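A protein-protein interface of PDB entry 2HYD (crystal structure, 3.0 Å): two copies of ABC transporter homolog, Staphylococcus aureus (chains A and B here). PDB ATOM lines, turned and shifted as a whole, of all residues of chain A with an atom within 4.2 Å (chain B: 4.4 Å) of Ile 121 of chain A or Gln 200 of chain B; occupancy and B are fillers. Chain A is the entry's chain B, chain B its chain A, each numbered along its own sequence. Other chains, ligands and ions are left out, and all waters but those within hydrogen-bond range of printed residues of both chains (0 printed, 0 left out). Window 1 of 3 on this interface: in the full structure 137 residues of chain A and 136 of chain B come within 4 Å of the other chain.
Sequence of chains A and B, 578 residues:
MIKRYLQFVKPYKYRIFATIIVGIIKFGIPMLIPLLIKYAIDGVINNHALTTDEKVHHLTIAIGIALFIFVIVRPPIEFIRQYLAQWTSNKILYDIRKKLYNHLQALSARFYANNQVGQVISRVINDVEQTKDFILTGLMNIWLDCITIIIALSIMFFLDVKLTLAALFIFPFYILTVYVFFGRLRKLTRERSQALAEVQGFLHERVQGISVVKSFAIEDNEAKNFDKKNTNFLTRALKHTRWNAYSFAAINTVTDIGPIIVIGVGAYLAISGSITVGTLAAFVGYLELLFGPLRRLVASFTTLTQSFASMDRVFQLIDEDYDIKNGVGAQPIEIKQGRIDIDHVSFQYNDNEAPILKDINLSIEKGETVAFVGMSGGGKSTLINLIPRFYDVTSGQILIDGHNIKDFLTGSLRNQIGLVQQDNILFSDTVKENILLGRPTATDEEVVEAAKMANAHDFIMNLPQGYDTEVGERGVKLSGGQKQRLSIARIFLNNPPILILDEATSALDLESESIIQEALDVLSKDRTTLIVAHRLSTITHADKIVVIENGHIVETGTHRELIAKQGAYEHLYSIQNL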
ATOM      1  N   VAL A 117     -22.884   0.850 -16.009  1.00  0.00           N
ATOM      2  CA  VAL A 117     -22.889   1.300 -14.636  1.00  0.00           C
ATOM      3  C   VAL A 117     -23.725   2.544 -14.419  1.00  0.00           C
ATOM      4  O   VAL A 117     -24.671   2.548 -13.623  1.00  0.00           O
ATOM      5  CB  VAL A 117     -21.486   1.618 -14.176  1.00  0.00           C
ATOM      6  CG1 VAL A 117     -21.511   2.065 -12.741  1.00  0.00           C
ATOM      7  CG2 VAL A 117     -20.619   0.409 -14.336  1.00  0.00           C
ATOM      8  N   GLY A 118     -23.361   3.607 -15.121  1.00  0.00           N
ATOM      9  CA  GLY A 118     -24.072   4.860 -14.975  1.00  0.00           C
ATOM     10  C   GLY A 118     -25.566   4.718 -15.116  1.00  0.00           C
ATOM     11  O   GLY A 118     -26.323   5.364 -14.397  1.00  0.00           O
ATOM     12  N   GLN A 119     -25.991   3.879 -16.059  1.00  0.00           N
ATOM     13  CA  GLN A 119     -27.405   3.655 -16.297  1.00  0.00           C
ATOM     14  C   GLN A 119     -28.021   2.959 -15.105  1.00  0.00           C
ATOM     15  O   GLN A 119     -29.073   3.363 -14.627  1.00  0.00           O
ATOM     16  CB  GLN A 119     -27.603   2.841 -17.564  1.00  0.00           C
ATOM     17  CG  GLN A 119     -28.154   3.674 -18.698  1.00  0.00           C
ATOM     18  CD  GLN A 119     -28.409   2.865 -19.945  1.00  0.00           C
ATOM     19  OE1 GLN A 119     -29.158   1.888 -19.926  1.00  0.00           O
ATOM     20  NE2 GLN A 119     -27.786   3.268 -21.045  1.00  0.00           N
ATOM     21  N   VAL A 120     -27.361   1.918 -14.613  1.00  0.00           N
ATOM     22  CA  VAL A 120     -27.851   1.210 -13.435  1.00  0.00           C
ATOM     23  C   VAL A 120     -28.005   2.199 -12.275  1.00  0.00           C
ATOM     24  O   VAL A 120     -29.096   2.335 -11.709  1.00  0.00           O
ATOM     25  CB  VAL A 120     -26.884   0.107 -12.999  1.00  0.00           C
ATOM     26  CG1 VAL A 120     -27.272  -0.413 -11.617  1.00  0.00           C
ATOM     27  CG2 VAL A 120     -26.912  -1.011 -14.010  1.00  0.00           C
ATOM     28  N   ILE A 121     -26.908   2.882 -11.930  1.00  0.00           N
ATOM     29  CA  ILE A 121     -26.924   3.867 -10.848  1.00  0.00           C
ATOM     30  C   ILE A 121     -28.081   4.860 -11.002  1.00  0.00           C
ATOM     31  O   ILE A 121     -28.803   5.140 -10.033  1.00  0.00           O
ATOM     32  CB  ILE A 121     -25.616   4.646 -10.794  1.00  0.00           C
ATOM     33  CG1 ILE A 121     -24.501   3.724 -10.332  1.00  0.00           C
ATOM     34  CG2 ILE A 121     -25.752   5.832  -9.867  1.00  0.00           C
ATOM     35  CD1 ILE A 121     -23.145   4.334 -10.468  1.00  0.00           C
ATOM     36  N   SER A 122     -28.263   5.400 -12.208  1.00  0.00           N
ATOM     37  CA  SER A 122     -29.352   6.347 -12.452  1.00  0.00           C
ATOM     38  C   SER A 122     -30.660   5.804 -11.847  1.00  0.00           C
ATOM     39  O   SER A 122     -31.428   6.548 -11.218  1.00  0.00           O
ATOM     40  CB  SER A 122     -29.522   6.581 -13.956  1.00  0.00           C
ATOM     41  OG  SER A 122     -30.665   7.379 -14.214  1.00  0.00           O
ATOM     42  N   ARG A 123     -30.896   4.505 -12.030  1.00  0.00           N
ATOM     43  CA  ARG A 123     -32.092   3.867 -11.502  1.00  0.00           C
ATOM     44  C   ARG A 123     -32.058   3.825  -9.990  1.00  0.00           C
ATOM     45  O   ARG A 123     -32.951   4.343  -9.326  1.00  0.00           O
ATOM     46  CB  ARG A 123     -32.223   2.457 -12.051  1.00  0.00           C
ATOM     47  CG  ARG A 123     -32.632   2.461 -13.479  1.00  0.00           C
ATOM     48  CD  ARG A 123     -32.918   1.094 -13.994  1.00  0.00           C
ATOM     49  NE  ARG A 123     -33.868   1.196 -15.088  1.00  0.00           N
ATOM     50  CZ  ARG A 123     -34.033   0.271 -16.022  1.00  0.00           C
ATOM     51  NH1 ARG A 123     -33.301  -0.840 -16.000  1.00  0.00           N
ATOM     52  NH2 ARG A 123     -34.929   0.460 -16.977  1.00  0.00           N
ATOM     53  N   VAL A 124     -31.017   3.210  -9.445  1.00  0.00           N
ATOM     54  CA  VAL A 124     -30.879   3.115  -8.005  1.00  0.00           C
ATOM     55  C   VAL A 124     -31.012   4.476  -7.321  1.00  0.00           C
ATOM     56  O   VAL A 124     -31.544   4.566  -6.216  1.00  0.00           O
ATOM     57  CB  VAL A 124     -29.542   2.478  -7.636  1.00  0.00           C
ATOM     58  CG1 VAL A 124     -29.200   2.787  -6.198  1.00  0.00           C
ATOM     59  CG2 VAL A 124     -29.629   0.977  -7.851  1.00  0.00           C
ATOM     60  N   ILE A 125     -30.575   5.542  -7.976  1.00  0.00           N
ATOM     61  CA  ILE A 125     -30.669   6.837  -7.340  1.00  0.00           C
ATOM     62  C   ILE A 125     -31.799   7.739  -7.783  1.00  0.00           C
ATOM     63  O   ILE A 125     -32.668   8.098  -6.982  1.00  0.00           O
ATOM     64  CB  ILE A 125     -29.362   7.589  -7.489  1.00  0.00           C
ATOM     65  CG1 ILE A 125     -28.296   6.896  -6.631  1.00  0.00           C
ATOM     66  CG2 ILE A 125     -29.566   9.076  -7.129  1.00  0.00           C
ATOM     67  CD1 ILE A 125     -26.934   7.502  -6.741  1.00  0.00           C
ATOM     68  N   HIS A 204     -20.245   8.469 -16.891  1.00  0.00           N
ATOM     69  CA  HIS A 204     -19.484   7.488 -16.134  1.00  0.00           C
ATOM     70  C   HIS A 204     -18.330   6.981 -16.987  1.00  0.00           C
ATOM     71  O   HIS A 204     -17.164   7.261 -16.708  1.00  0.00           O
ATOM     72  CB  HIS A 204     -20.371   6.309 -15.705  1.00  0.00           C
ATOM     73  CG  HIS A 204     -21.148   6.551 -14.443  1.00  0.00           C
ATOM     74  ND1 HIS A 204     -20.866   5.909 -13.255  1.00  0.00           N
ATOM     75  CD2 HIS A 204     -22.194   7.371 -14.187  1.00  0.00           C
ATOM     76  CE1 HIS A 204     -21.706   6.327 -12.323  1.00  0.00           C
ATOM     77  NE2 HIS A 204     -22.523   7.213 -12.862  1.00  0.00           N
ATOM     78  N   GLY B 118     -18.305   8.960  -9.550  1.00  0.00           N
ATOM     79  CA  GLY B 118     -19.682   9.060  -9.113  1.00  0.00           C
ATOM     80  C   GLY B 118     -20.008  10.391  -8.469  1.00  0.00           C
ATOM     81  O   GLY B 118     -21.087  10.940  -8.679  1.00  0.00           O
ATOM     82  N   SER B 122     -22.582  13.132  -9.909  1.00  0.00           N
ATOM     83  CA  SER B 122     -23.675  13.596  -9.054  1.00  0.00           C
ATOM     84  C   SER B 122     -23.866  15.118  -9.238  1.00  0.00           C
ATOM     85  O   SER B 122     -25.001  15.612  -9.325  1.00  0.00           O
ATOM     86  CB  SER B 122     -23.376  13.272  -7.585  1.00  0.00           C
ATOM     87  OG  SER B 122     -24.364  13.832  -6.736  1.00  0.00           O
ATOM     88  N   ASN B 126     -27.282  15.752 -10.772  1.00  0.00           N
ATOM     89  CA  ASN B 126     -28.180  16.093  -9.680  1.00  0.00           C
ATOM     90  C   ASN B 126     -28.138  17.555  -9.251  1.00  0.00           C
ATOM     91  O   ASN B 126     -29.164  18.248  -9.284  1.00  0.00           O
ATOM     92  CB  ASN B 126     -27.888  15.178  -8.494  1.00  0.00           C
ATOM     93  CG  ASN B 126     -28.171  13.729  -8.812  1.00  0.00           C
ATOM     94  OD1 ASN B 126     -29.316  13.320  -8.995  1.00  0.00           O
ATOM     95  ND2 ASN B 126     -27.120  12.940  -8.869  1.00  0.00           N
ATOM     96  N   LEU B 196     -25.376  12.443  -0.869  1.00  0.00           N
ATOM     97  CA  LEU B 196     -25.901  11.748  -2.025  1.00  0.00           C
ATOM     98  C   LEU B 196     -24.716  11.465  -2.915  1.00  0.00           C
ATOM     99  O   LEU B 196     -24.470  10.329  -3.310  1.00  0.00           O
ATOM    100  CB  LEU B 196     -26.876  12.636  -2.771  1.00  0.00           C
ATOM    101  CG  LEU B 196     -27.505  11.892  -3.935  1.00  0.00           C
ATOM    102  CD1 LEU B 196     -28.253  10.680  -3.394  1.00  0.00           C
ATOM    103  CD2 LEU B 196     -28.445  12.822  -4.679  1.00  0.00           C
ATOM    104  N   ALA B 197     -23.969  12.530  -3.194  1.00  0.00           N
ATOM    105  CA  ALA B 197     -22.785  12.467  -4.040  1.00  0.00           C
ATOM    106  C   ALA B 197     -21.896  11.297  -3.658  1.00  0.00           C
ATOM    107  O   ALA B 197     -21.414  10.555  -4.525  1.00  0.00           O
ATOM    108  CB  ALA B 197     -22.010  13.763  -3.935  1.00  0.00           C
ATOM    109  N   GLU B 198     -21.690  11.126  -2.357  1.00  0.00           N
ATOM    110  CA  GLU B 198     -20.849  10.052  -1.861  1.00  0.00           C
ATOM    111  C   GLU B 198     -21.474   8.680  -2.070  1.00  0.00           C
ATOM    112  O   GLU B 198     -20.752   7.706  -2.275  1.00  0.00           O
ATOM    113  CB  GLU B 198     -20.514  10.291  -0.390  1.00  0.00           C
ATOM    114  CG  GLU B 198     -19.700  11.553  -0.169  1.00  0.00           C
ATOM    115  CD  GLU B 198     -19.540  11.896   1.296  1.00  0.00           C
ATOM    116  OE1 GLU B 198     -20.561  12.154   1.976  1.00  0.00           O
ATOM    117  OE2 GLU B 198     -18.388  11.906   1.769  1.00  0.00           O
ATOM    118  N   VAL B 199     -22.798   8.571  -2.018  1.00  0.00           N
ATOM    119  CA  VAL B 199     -23.373   7.259  -2.264  1.00  0.00           C
ATOM    120  C   VAL B 199     -23.172   6.988  -3.750  1.00  0.00           C
ATOM    121  O   VAL B 199     -22.884   5.853  -4.140  1.00  0.00           O
ATOM    122  CB  VAL B 199     -24.867   7.187  -1.910  1.00  0.00           C
ATOM    123  CG1 VAL B 199     -25.169   8.174  -0.793  1.00  0.00           C
ATOM    124  CG2 VAL B 199     -25.724   7.430  -3.142  1.00  0.00           C
ATOM    125  N   GLN B 200     -23.328   8.033  -4.571  1.00  0.00           N
ATOM    126  CA  GLN B 200     -23.112   7.940  -6.016  1.00  0.00           C
ATOM    127  C   GLN B 200     -21.722   7.346  -6.168  1.00  0.00           C
ATOM    128  O   GLN B 200     -21.536   6.246  -6.693  1.00  0.00           O
ATOM    129  CB  GLN B 200     -23.080   9.329  -6.657  1.00  0.00           C
ATOM    130  CG  GLN B 200     -24.412  10.044  -6.834  1.00  0.00           C
ATOM    131  CD  GLN B 200     -25.004   9.849  -8.214  1.00  0.00           C
ATOM    132  OE1 GLN B 200     -26.138  10.242  -8.481  1.00  0.00           O
ATOM    133  NE2 GLN B 200     -24.240   9.219  -9.092  1.00  0.00           N
ATOM    134  N   GLY B 201     -20.737   8.090  -5.684  1.00  0.00           N
ATOM    135  CA  GLY B 201     -19.365   7.638  -5.784  1.00  0.00           C
ATOM    136  C   GLY B 201     -19.164   6.205  -5.359  1.00  0.00           C
ATOM    137  O   GLY B 201     -18.392   5.492  -5.986  1.00  0.00           O
ATOM    138  N   PHE B 202     -19.848   5.781  -4.300  1.00  0.00           N
ATOM    139  CA  PHE B 202     -19.698   4.422  -3.816  1.00  0.00           C
ATOM    140  C   PHE B 202     -20.233   3.451  -4.841  1.00  0.00           C
ATOM    141  O   PHE B 202     -19.520   2.563  -5.307  1.00  0.00           O
ATOM    142  CB  PHE B 202     -20.449   4.220  -2.505  1.00  0.00           C
ATOM    143  CG  PHE B 202     -20.177   2.892  -1.860  1.00  0.00           C
ATOM    144  CD1 PHE B 202     -19.006   2.683  -1.148  1.00  0.00           C
ATOM    145  CD2 PHE B 202     -21.051   1.828  -2.033  1.00  0.00           C
ATOM    146  CE1 PHE B 202     -18.704   1.433  -0.626  1.00  0.00           C
ATOM    147  CE2 PHE B 202     -20.753   0.583  -1.513  1.00  0.00           C
ATOM    148  CZ  PHE B 202     -19.573   0.385  -0.808  1.00  0.00           C
ATOM    149  N   LEU B 203     -21.499   3.624  -5.194  1.00  0.00           N
ATOM    150  CA  LEU B 203     -22.135   2.746  -6.163  1.00  0.00           C
ATOM    151  C   LEU B 203     -21.282   2.588  -7.412  1.00  0.00           C
ATOM    152  O   LEU B 203     -21.045   1.472  -7.871  1.00  0.00           O
ATOM    153  CB  LEU B 203     -23.515   3.277  -6.534  1.00  0.00           C
ATOM    154  CG  LEU B 203     -24.554   3.190  -5.421  1.00  0.00           C
ATOM    155  CD1 LEU B 203     -25.818   3.930  -5.820  1.00  0.00           C
ATOM    156  CD2 LEU B 203     -24.842   1.733  -5.138  1.00  0.00           C
ATOM    157  N   HIS B 204     -20.819   3.700  -7.964  1.00  0.00           N
ATOM    158  CA  HIS B 204     -19.994   3.631  -9.156  1.00  0.00           C
ATOM    159  C   HIS B 204     -18.849   2.646  -8.922  1.00  0.00           C
ATOM    160  O   HIS B 204     -18.807   1.550  -9.490  1.00  0.00           O
ATOM    161  CB  HIS B 204     -19.449   5.024  -9.488  1.00  0.00           C
ATOM    162  CG  HIS B 204     -18.410   5.031 -10.566  1.00  0.00           C
ATOM    163  ND1 HIS B 204     -17.058   4.986 -10.298  1.00  0.00           N
ATOM    164  CD2 HIS B 204     -18.521   5.096 -11.913  1.00  0.00           C
ATOM    165  CE1 HIS B 204     -16.385   5.024 -11.433  1.00  0.00           C
ATOM    166  NE2 HIS B 204     -17.249   5.091 -12.428  1.00  0.00           N
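Ile 121 of chain A touches three residues of chain B.
Arg 123 of chain A touches none of the printed residues of chain B.
Of the printed residues of chain B, Val 124 of chain A touches Leu 203 (3.6 Å).
Of the printed residues of chain B, His 204 of chain A touches His 204 (2.8 Å).
Of the printed residues of chain A, Gln 200 of chain B touches Ile 121 and Ile 125.
Gly 201 of chain B touches none of the printed residues of chain A.
The nearest printed residue of chain B that does not touch His 204 of chain A is Gln 200 of chain B (4.6 Å).
Among the printed residues, merely in contact across the chains: His 204 of chain A with His 204 of chain B (2.8 Å), Ile 125 of chain A with Gln 200 of chain B (3.3 Å), Ile 121 of chain A with His 204 of chain B (3.5 Å), Val 124 of chain A with Leu 203 of chain B (3.6 Å), Ile 121 of chain A with Gln 200 of chain B (3.8 Å), Ile 125 of chain A with Val 199 of chain B (3.8 Å), Ile 125 of chain A with Leu 203 of chain B (3.9 Å) and Ile 121 of chain A with Leu 203 of chain B (3.9 Å).
His 204 of chain B touches its own counterpart, His 204 of chain A.
Of the 8 pairs that touch across the chains among the printed residues, 1 has its exchanged pair printed and touching as well.
The side-chain amide oxygen of Gln 200 of chain B sits at hydrogen-bond distance from the side-chain amide nitrogen of Asn 126 of chain B (2.9 Å).
Of the 10 printed residues of chain A, 4 touch a printed residue of chain B.
Printed residues of chain A that touch a printed residue of chain B: Ile 121, Val 124, Ile 125 and His 204.
Hydrophobic or aromatic side chains of chain A within 4 Å of the printed part of chain B: Ile 121, Val 124, Ile 125 and His 204.
Of the 12 printed residues of chain B, 4 touch a printed residue of chain A.
Along chain B the printed residues that touch a printed residue of chain A span positions 199 to 204.
Among the printed residues, no Asp or Glu carboxylate lies within 4 Å of a Lys or Arg side-chain nitrogen of the other chain.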
